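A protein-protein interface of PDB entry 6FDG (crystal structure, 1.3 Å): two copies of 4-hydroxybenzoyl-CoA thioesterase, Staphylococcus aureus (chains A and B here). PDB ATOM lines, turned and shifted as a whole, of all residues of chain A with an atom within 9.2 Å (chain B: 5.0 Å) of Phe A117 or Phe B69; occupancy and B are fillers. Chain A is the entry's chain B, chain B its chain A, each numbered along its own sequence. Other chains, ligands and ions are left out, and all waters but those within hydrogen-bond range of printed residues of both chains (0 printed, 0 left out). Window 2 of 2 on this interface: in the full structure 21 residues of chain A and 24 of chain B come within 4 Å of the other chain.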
ATOM      1  N   GLU A  49      11.538  -4.980  -0.091  1.00  0.00           N
ATOM      2  CA  GLU A  49      12.668  -5.730   0.501  1.00  0.00           C
ATOM      3  C   GLU A  49      13.746  -4.781   0.868  1.00  0.00           C
ATOM      4  O   GLU A  49      14.291  -4.925   1.969  1.00  0.00           O
ATOM      5  CB  GLU A  49      13.186  -6.916  -0.356  1.00  0.00           C
ATOM      6  CG  GLU A  49      12.185  -8.045  -0.437  1.00  0.00           C
ATOM      7  CD  GLU A  49      12.847  -9.411  -0.786  1.00  0.00           C
ATOM      8  OE1 GLU A  49      12.379 -10.514  -0.319  1.00  0.00           O
ATOM      9  OE2 GLU A  49      13.860  -9.327  -1.472  1.00  0.00           O
ATOM     10  N   GLY A  52      13.328  -3.607   4.527  1.00  0.00           N
ATOM     11  CA  GLY A  52      13.345  -4.593   5.674  1.00  0.00           C
ATOM     12  C   GLY A  52      12.053  -5.392   5.944  1.00  0.00           C
ATOM     13  O   GLY A  52      11.800  -5.932   7.066  1.00  0.00           O
ATOM     14  N   ILE A  53      11.151  -5.327   4.943  1.00  0.00           N
ATOM     15  CA  ILE A  53       9.840  -6.041   5.007  1.00  0.00           C
ATOM     16  C   ILE A  53       9.869  -7.091   3.852  1.00  0.00           C
ATOM     17  O   ILE A  53      10.260  -6.797   2.714  1.00  0.00           O
ATOM     18  CB  ILE A  53       8.618  -5.106   4.860  1.00  0.00           C
ATOM     19  CG1 ILE A  53       8.582  -4.095   6.017  1.00  0.00           C
ATOM     20  CG2 ILE A  53       7.335  -5.958   4.967  1.00  0.00           C
ATOM     21  CD1 ILE A  53       8.556  -4.678   7.396  1.00  0.00           C
ATOM     22  N   ILE A  54       9.423  -8.314   4.250  1.00  0.00           N
ATOM     23  CA  ILE A  54       9.449  -9.432   3.296  1.00  0.00           C
ATOM     24  C   ILE A  54       8.068  -9.936   3.353  1.00  0.00           C
ATOM     25  O   ILE A  54       7.288  -9.800   4.261  1.00  0.00           O
ATOM     26  CB  ILE A  54      10.532 -10.493   3.593  1.00  0.00           C
ATOM     27  CG1 ILE A  54      10.319 -11.079   4.991  1.00  0.00           C
ATOM     28  CG2 ILE A  54      11.929  -9.924   3.294  1.00  0.00           C
ATOM     29  CD1 ILE A  54      11.433 -12.027   5.406  1.00  0.00           C
ATOM     30  N   SER A  55       7.800 -10.739   2.275  1.00  0.00           N
ATOM     31  CA  SER A  55       6.448 -11.241   2.018  1.00  0.00           C
ATOM     32  C   SER A  55       6.505 -12.778   1.741  1.00  0.00           C
ATOM     33  O   SER A  55       6.503 -13.147   0.576  1.00  0.00           O
ATOM     34  CB  SER A  55       5.821 -10.538   0.821  1.00  0.00           C
ATOM     35  OG  SER A  55       4.495 -10.884   0.843  1.00  0.00           O
ATOM     36  N   PRO A  56       6.503 -13.574   2.789  1.00  0.00           N
ATOM     37  CA  PRO A  56       6.462 -15.027   2.563  1.00  0.00           C
ATOM     38  C   PRO A  56       5.090 -15.547   2.163  1.00  0.00           C
ATOM     39  O   PRO A  56       4.045 -15.102   2.580  1.00  0.00           O
ATOM     40  CB  PRO A  56       6.825 -15.623   3.930  1.00  0.00           C
ATOM     41  CG  PRO A  56       6.371 -14.549   4.940  1.00  0.00           C
ATOM     42  CD  PRO A  56       6.495 -13.226   4.238  1.00  0.00           C
ATOM     43  N   VAL A  57       5.175 -16.744   1.486  1.00  0.00           N
ATOM     44  CA  VAL A  57       4.010 -17.503   1.101  1.00  0.00           C
ATOM     45  C   VAL A  57       3.619 -18.307   2.305  1.00  0.00           C
ATOM     46  O   VAL A  57       4.485 -19.007   2.941  1.00  0.00           O
ATOM     47  CB  VAL A  57       4.320 -18.427  -0.108  1.00  0.00           C
ATOM     48  CG1 VAL A  57       3.190 -19.390  -0.340  1.00  0.00           C
ATOM     49  CG2 VAL A  57       4.613 -17.609  -1.324  1.00  0.00           C
ATOM     50  N   ILE A 110       1.654 -13.102   3.424  1.00  0.00           N
ATOM     51  CA  ILE A 110       1.589 -12.066   4.508  1.00  0.00           C
ATOM     52  C   ILE A 110       2.821 -11.235   4.335  1.00  0.00           C
ATOM     53  O   ILE A 110       3.726 -11.415   3.611  1.00  0.00           O
ATOM     54  CB  ILE A 110       1.573 -12.799   5.873  1.00  0.00           C
ATOM     55  CG1 ILE A 110       2.821 -13.524   6.145  1.00  0.00           C
ATOM     56  CG2 ILE A 110       0.387 -13.611   6.076  1.00  0.00           C
ATOM     57  CD1 ILE A 110       2.965 -14.071   7.561  1.00  0.00           C
ATOM     58  N   CYS A 111       2.934 -10.172   5.229  1.00  0.00           N
ATOM     59  CA  CYS A 111       4.150  -9.343   5.256  1.00  0.00           C
ATOM     60  C   CYS A 111       4.718  -9.340   6.723  1.00  0.00           C
ATOM     61  O   CYS A 111       3.894  -9.298   7.627  1.00  0.00           O
ATOM     62  CB  CYS A 111       3.834  -7.859   4.868  1.00  0.00           C
ATOM     63  SG  CYS A 111       3.574  -7.632   3.080  1.00  0.00           S
ATOM     64  N   ILE A 112       6.006  -9.492   6.791  1.00  0.00           N
ATOM     65  CA  ILE A 112       6.649  -9.659   8.123  1.00  0.00           C
ATOM     66  C   ILE A 112       7.900  -8.819   8.147  1.00  0.00           C
ATOM     67  O   ILE A 112       8.476  -8.431   7.122  1.00  0.00           O
ATOM     68  CB  ILE A 112       6.978 -11.149   8.431  1.00  0.00           C
ATOM     69  CG1 ILE A 112       8.012 -11.667   7.501  1.00  0.00           C
ATOM     70  CG2 ILE A 112       5.745 -12.013   8.468  1.00  0.00           C
ATOM     71  CD1 ILE A 112       8.517 -13.087   7.866  1.00  0.00           C
ATOM     72  N   LYS A 113       8.351  -8.403   9.365  1.00  0.00           N
ATOM     73  CA  LYS A 113       9.645  -7.737   9.413  1.00  0.00           C
ATOM     74  C   LYS A 113      10.726  -8.758   9.263  1.00  0.00           C
ATOM     75  O   LYS A 113      10.666  -9.824   9.857  1.00  0.00           O
ATOM     76  CB  LYS A 113       9.815  -7.013  10.803  1.00  0.00           C
ATOM     77  CG  LYS A 113       8.681  -6.054  11.096  1.00  0.00           C
ATOM     78  CD  LYS A 113       8.828  -5.259  12.398  1.00  0.00           C
ATOM     79  CE  LYS A 113       9.857  -4.138  12.260  1.00  0.00           C
ATOM     80  NZ  LYS A 113       9.255  -2.817  12.608  1.00  0.00           N
ATOM     81  N   GLU A 114      11.671  -8.459   8.411  1.00  0.00           N
ATOM     82  CA  GLU A 114      12.793  -9.321   8.106  1.00  0.00           C
ATOM     83  C   GLU A 114      13.696  -9.683   9.298  1.00  0.00           C
ATOM     84  O   GLU A 114      14.150 -10.836   9.400  1.00  0.00           O
ATOM     85  CB  GLU A 114      13.602  -8.648   7.016  1.00  0.00           C
ATOM     86  CG  GLU A 114      14.773  -9.465   6.475  1.00  0.00           C
ATOM     87  CD  GLU A 114      15.629  -8.641   5.581  1.00  0.00           C
ATOM     88  OE1 GLU A 114      15.076  -7.727   4.952  1.00  0.00           O
ATOM     89  OE2 GLU A 114      16.847  -8.890   5.503  1.00  0.00           O
ATOM     90  N   ASP A 115      13.955  -8.716  10.185  1.00  0.00           N
ATOM     91  CA  ASP A 115      14.724  -8.998  11.441  1.00  0.00           C
ATOM     92  C   ASP A 115      13.920  -9.954  12.328  1.00  0.00           C
ATOM     93  O   ASP A 115      14.264 -11.128  12.480  1.00  0.00           O
ATOM     94  CB  ASP A 115      15.204  -7.724  12.205  1.00  0.00           C
ATOM     95  CG  ASP A 115      14.262  -6.478  12.063  1.00  0.00           C
ATOM     96  OD1 ASP A 115      13.026  -6.618  12.065  1.00  0.00           O
ATOM     97  OD2 ASP A 115      14.783  -5.336  11.994  1.00  0.00           O
ATOM     98  N   THR A 116      12.804  -9.451  12.828  1.00  0.00           N
ATOM     99  CA  THR A 116      11.915 -10.180  13.719  1.00  0.00           C
ATOM    100  C   THR A 116      11.217 -11.449  13.152  1.00  0.00           C
ATOM    101  O   THR A 116      10.881 -12.358  13.904  1.00  0.00           O
ATOM    102  CB  THR A 116      10.853  -9.185  14.211  1.00  0.00           C
ATOM    103  OG1 THR A 116      11.513  -7.972  14.587  1.00  0.00           O
ATOM    104  CG2 THR A 116      10.089  -9.722  15.399  1.00  0.00           C
ATOM    105  N   PHE A 117      10.961 -11.518  11.853  1.00  0.00           N
ATOM    106  CA  PHE A 117       9.950 -12.474  11.326  1.00  0.00           C
ATOM    107  C   PHE A 117       8.505 -12.289  11.911  1.00  0.00           C
ATOM    108  O   PHE A 117       7.602 -13.081  11.614  1.00  0.00           O
ATOM    109  CB  PHE A 117      10.464 -13.958  11.315  1.00  0.00           C
ATOM    110  CG  PHE A 117      11.219 -14.351  10.007  1.00  0.00           C
ATOM    111  CD1 PHE A 117      12.328 -13.603   9.539  1.00  0.00           C
ATOM    112  CD2 PHE A 117      10.827 -15.463   9.252  1.00  0.00           C
ATOM    113  CE1 PHE A 117      12.985 -13.932   8.339  1.00  0.00           C
ATOM    114  CE2 PHE A 117      11.485 -15.797   8.047  1.00  0.00           C
ATOM    115  CZ  PHE A 117      12.585 -15.051   7.606  1.00  0.00           C
ATOM    116  N   LYS A 118       8.257 -11.155  12.587  1.00  0.00           N
ATOM    117  CA  LYS A 118       6.915 -10.804  13.143  1.00  0.00           C
ATOM    118  C   LYS A 118       5.963 -10.227  12.027  1.00  0.00           C
ATOM    119  O   LYS A 118       6.418  -9.348  11.365  1.00  0.00           O
ATOM    120  CB  LYS A 118       7.089  -9.747  14.260  1.00  0.00           C
ATOM    121  CG  LYS A 118       5.819  -9.120  14.847  1.00  0.00           C
ATOM    122  CD  LYS A 118       5.020 -10.100  15.711  1.00  0.00           C
ATOM    123  CE  LYS A 118       3.549  -9.712  15.826  1.00  0.00           C
ATOM    124  NZ  LYS A 118       2.880 -10.492  16.901  1.00  0.00           N
ATOM    125  N   PRO A 119       4.662 -10.676  11.942  1.00  0.00           N
ATOM    126  CA  PRO A 119       3.768 -10.135  10.948  1.00  0.00           C
ATOM    127  C   PRO A 119       3.445  -8.636  11.133  1.00  0.00           C
ATOM    128  O   PRO A 119       3.765  -8.005  12.154  1.00  0.00           O
ATOM    129  CB  PRO A 119       2.501 -10.999  11.025  1.00  0.00           C
ATOM    130  CG  PRO A 119       2.834 -12.157  11.825  1.00  0.00           C
ATOM    131  CD  PRO A 119       4.067 -11.833  12.635  1.00  0.00           C
ATOM    132  N   ILE A 120       2.865  -8.043  10.114  1.00  0.00           N
ATOM    133  CA  ILE A 120       2.681  -6.591  10.133  1.00  0.00           C
ATOM    134  C   ILE A 120       1.443  -6.297   9.310  1.00  0.00           C
ATOM    135  O   ILE A 120       0.999  -7.056   8.434  1.00  0.00           O
ATOM    136  CB  ILE A 120       3.945  -5.764   9.618  1.00  0.00           C
ATOM    137  CG1 ILE A 120       4.287  -6.043   8.145  1.00  0.00           C
ATOM    138  CG2 ILE A 120       5.190  -5.981  10.460  1.00  0.00           C
ATOM    139  CD1 ILE A 120       4.025  -4.929   7.144  1.00  0.00           C
ATOM    140  N   MET B  18      15.883 -14.714   1.175  1.00  0.00           N
ATOM    141  CA  MET B  18      15.469 -14.604   2.656  1.00  0.00           C
ATOM    142  C   MET B  18      16.318 -15.560   3.656  1.00  0.00           C
ATOM    143  O   MET B  18      16.215 -15.443   4.941  1.00  0.00           O
ATOM    144  CB  MET B  18      13.922 -14.650   2.881  1.00  0.00           C
ATOM    145  CG  MET B  18      12.809 -14.332   1.807  1.00  0.00           C
ATOM    146  SD  MET B  18      10.910 -14.450   2.150  1.00  0.00           S
ATOM    147  CE  MET B  18      11.146 -15.257   3.730  1.00  0.00           C
ATOM    148  N   GLY B  19      17.187 -16.498   3.220  1.00  0.00           N
ATOM    149  CA  GLY B  19      17.870 -17.492   3.996  1.00  0.00           C
ATOM    150  C   GLY B  19      17.045 -18.653   4.485  1.00  0.00           C
ATOM    151  O   GLY B  19      17.485 -19.581   5.240  1.00  0.00           O
ATOM    152  N   VAL B  20      15.851 -18.773   3.897  1.00  0.00           N
ATOM    153  CA  VAL B  20      14.924 -19.845   4.253  1.00  0.00           C
ATOM    154  C   VAL B  20      14.881 -20.823   3.004  1.00  0.00           C
ATOM    155  O   VAL B  20      15.296 -20.458   1.938  1.00  0.00           O
ATOM    156  CB  VAL B  20      13.538 -19.358   4.570  1.00  0.00           C
ATOM    157  CG1 VAL B  20      13.526 -18.316   5.728  1.00  0.00           C
ATOM    158  CG2 VAL B  20      12.780 -18.793   3.441  1.00  0.00           C
ATOM    159  N   SER B  67       8.880 -20.817   8.905  1.00  0.00           N
ATOM    160  CA  SER B  67      10.022 -20.896   8.007  1.00  0.00           C
ATOM    161  C   SER B  67      11.024 -21.944   8.396  1.00  0.00           C
ATOM    162  O   SER B  67      11.210 -22.231   9.670  1.00  0.00           O
ATOM    163  CB  SER B  67      10.661 -19.490   7.715  1.00  0.00           C
ATOM    164  OG  SER B  67       9.742 -18.718   6.989  1.00  0.00           O
ATOM    165  N   ILE B  68      11.701 -22.596   7.496  1.00  0.00           N
ATOM    166  CA  ILE B  68      12.821 -23.504   7.736  1.00  0.00           C
ATOM    167  C   ILE B  68      14.080 -22.783   7.297  1.00  0.00           C
ATOM    168  O   ILE B  68      14.247 -22.403   6.093  1.00  0.00           O
ATOM    169  CB  ILE B  68      12.594 -24.906   7.076  1.00  0.00           C
ATOM    170  CG1 ILE B  68      11.287 -25.512   7.641  1.00  0.00           C
ATOM    171  CG2 ILE B  68      13.739 -25.822   7.222  1.00  0.00           C
ATOM    172  CD1 ILE B  68      10.843 -26.814   7.001  1.00  0.00           C
ATOM    173  N   PHE B  69      14.918 -22.396   8.318  1.00  0.00           N
ATOM    174  CA  PHE B  69      16.178 -21.695   8.045  1.00  0.00           C
ATOM    175  C   PHE B  69      17.251 -22.721   7.872  1.00  0.00           C
ATOM    176  O   PHE B  69      17.409 -23.665   8.638  1.00  0.00           O
ATOM    177  CB  PHE B  69      16.511 -20.798   9.185  1.00  0.00           C
ATOM    178  CG  PHE B  69      15.574 -19.571   9.318  1.00  0.00           C
ATOM    179  CD1 PHE B  69      14.422 -19.700  10.043  1.00  0.00           C
ATOM    180  CD2 PHE B  69      15.914 -18.376   8.736  1.00  0.00           C
ATOM    181  CE1 PHE B  69      13.557 -18.630  10.174  1.00  0.00           C
ATOM    182  CE2 PHE B  69      15.084 -17.234   8.884  1.00  0.00           C
ATOM    183  CZ  PHE B  69      13.887 -17.415   9.580  1.00  0.00           C
ATOM    184  N   TYR B  70      18.013 -22.632   6.793  1.00  0.00           N
ATOM    185  CA  TYR B  70      19.130 -23.478   6.520  1.00  0.00           C
ATOM    186  C   TYR B  70      20.389 -23.093   7.556  1.00  0.00           C
ATOM    187  O   TYR B  70      20.548 -21.912   7.839  1.00  0.00           O
ATOM    188  CB  TYR B  70      19.599 -23.148   5.108  1.00  0.00           C
ATOM    189  CG  TYR B  70      20.889 -23.837   4.788  1.00  0.00           C
ATOM    190  CD1 TYR B  70      20.933 -25.113   4.327  1.00  0.00           C
ATOM    191  CD2 TYR B  70      22.142 -23.224   5.126  1.00  0.00           C
ATOM    192  CE1 TYR B  70      22.116 -25.784   4.153  1.00  0.00           C
ATOM    193  CE2 TYR B  70      23.327 -23.877   4.902  1.00  0.00           C
ATOM    194  CZ  TYR B  70      23.250 -25.169   4.301  1.00  0.00           C
ATOM    195  OH  TYR B  70      24.428 -25.799   4.154  1.00  0.00           O
ATOM    196  N   PRO B  71      21.143 -24.051   7.959  1.00  0.00           N
ATOM    197  CA  PRO B  71      21.061 -25.472   7.819  1.00  0.00           C
ATOM    198  C   PRO B  71      19.876 -26.078   8.665  1.00  0.00           C
ATOM    199  O   PRO B  71      19.464 -25.481   9.708  1.00  0.00           O
ATOM    200  CB  PRO B  71      22.402 -25.995   8.235  1.00  0.00           C
ATOM    201  CG  PRO B  71      22.771 -25.043   9.288  1.00  0.00           C
ATOM    202  CD  PRO B  71      22.247 -23.688   8.894  1.00  0.00           C
ATOM    203  N   GLU B  72      19.385 -27.263   8.324  1.00  0.00           N
ATOM    204  CA  GLU B  72      18.367 -27.937   9.142  1.00  0.00           C
ATOM    205  C   GLU B  72      18.213 -29.345   8.753  1.00  0.00           C
ATOM    206  O   GLU B  72      18.088 -29.654   7.525  1.00  0.00           O
ATOM    207  CB  GLU B  72      16.982 -27.280   8.931  1.00  0.00           C
ATOM    208  CG  GLU B  72      15.893 -27.510   9.959  1.00  0.00           C
ATOM    209  CD  GLU B  72      15.826 -26.477  11.077  1.00  0.00           C
ATOM    210  OE1 GLU B  72      16.418 -25.433  11.005  1.00  0.00           O
ATOM    211  OE2 GLU B  72      15.173 -26.735  12.063  1.00  0.00           O
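Of the printed residues of chain B, Ile A54 touches Met B18 (3.7 Å).
Phe A117 touches just these residues of chain B: Val B20, Ser B67 and Phe B69.
Of the printed residues of chain A, Val B20 touches Phe A117 (3.9 Å).
Of the printed residues of chain A, Ser B67 touches Phe A117 (3.6 Å).
Phe B69 touches one residue of chain A.
The nearest residue of chain B that does not touch Phe A117 is Met B18 (4.1 Å).
The nearest residue of chain A that does not touch Phe B69 is Glu A114 (6.5 Å).
The nearest printed residue of chain A that does not touch Ser B67 is Pro A56 (5.2 Å).
The backbone carbonyl oxygen of Ile A54 sits at hydrogen-bond distance from the backbone NH of Ile A112 (2.9 Å).
Of the 9 printed residues of chain B, 4 touch a printed residue of chain A.
Hydrophobic or aromatic side chains of chain B that line the printed part of chain A: Met B18, Val B20 and Phe B69.
Along chain B the printed residues that touch a printed residue of chain A span positions 18 to 69.
Of the 18 printed residues of chain A, 2 touch a printed residue of chain B.
Hydrophobic or aromatic side chains of chain A within 4 Å of the printed part of chain B: Ile A54 and Phe A117.
Among the printed residues, 4 pairs touch across the chains.
No position is printed for both chains.
Among the printed residues, merely in contact across the chains: Phe A117 with Phe B69, Phe A117 with Ser B67, Ile A54 with Met B18 and Phe A117 with Val B20.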
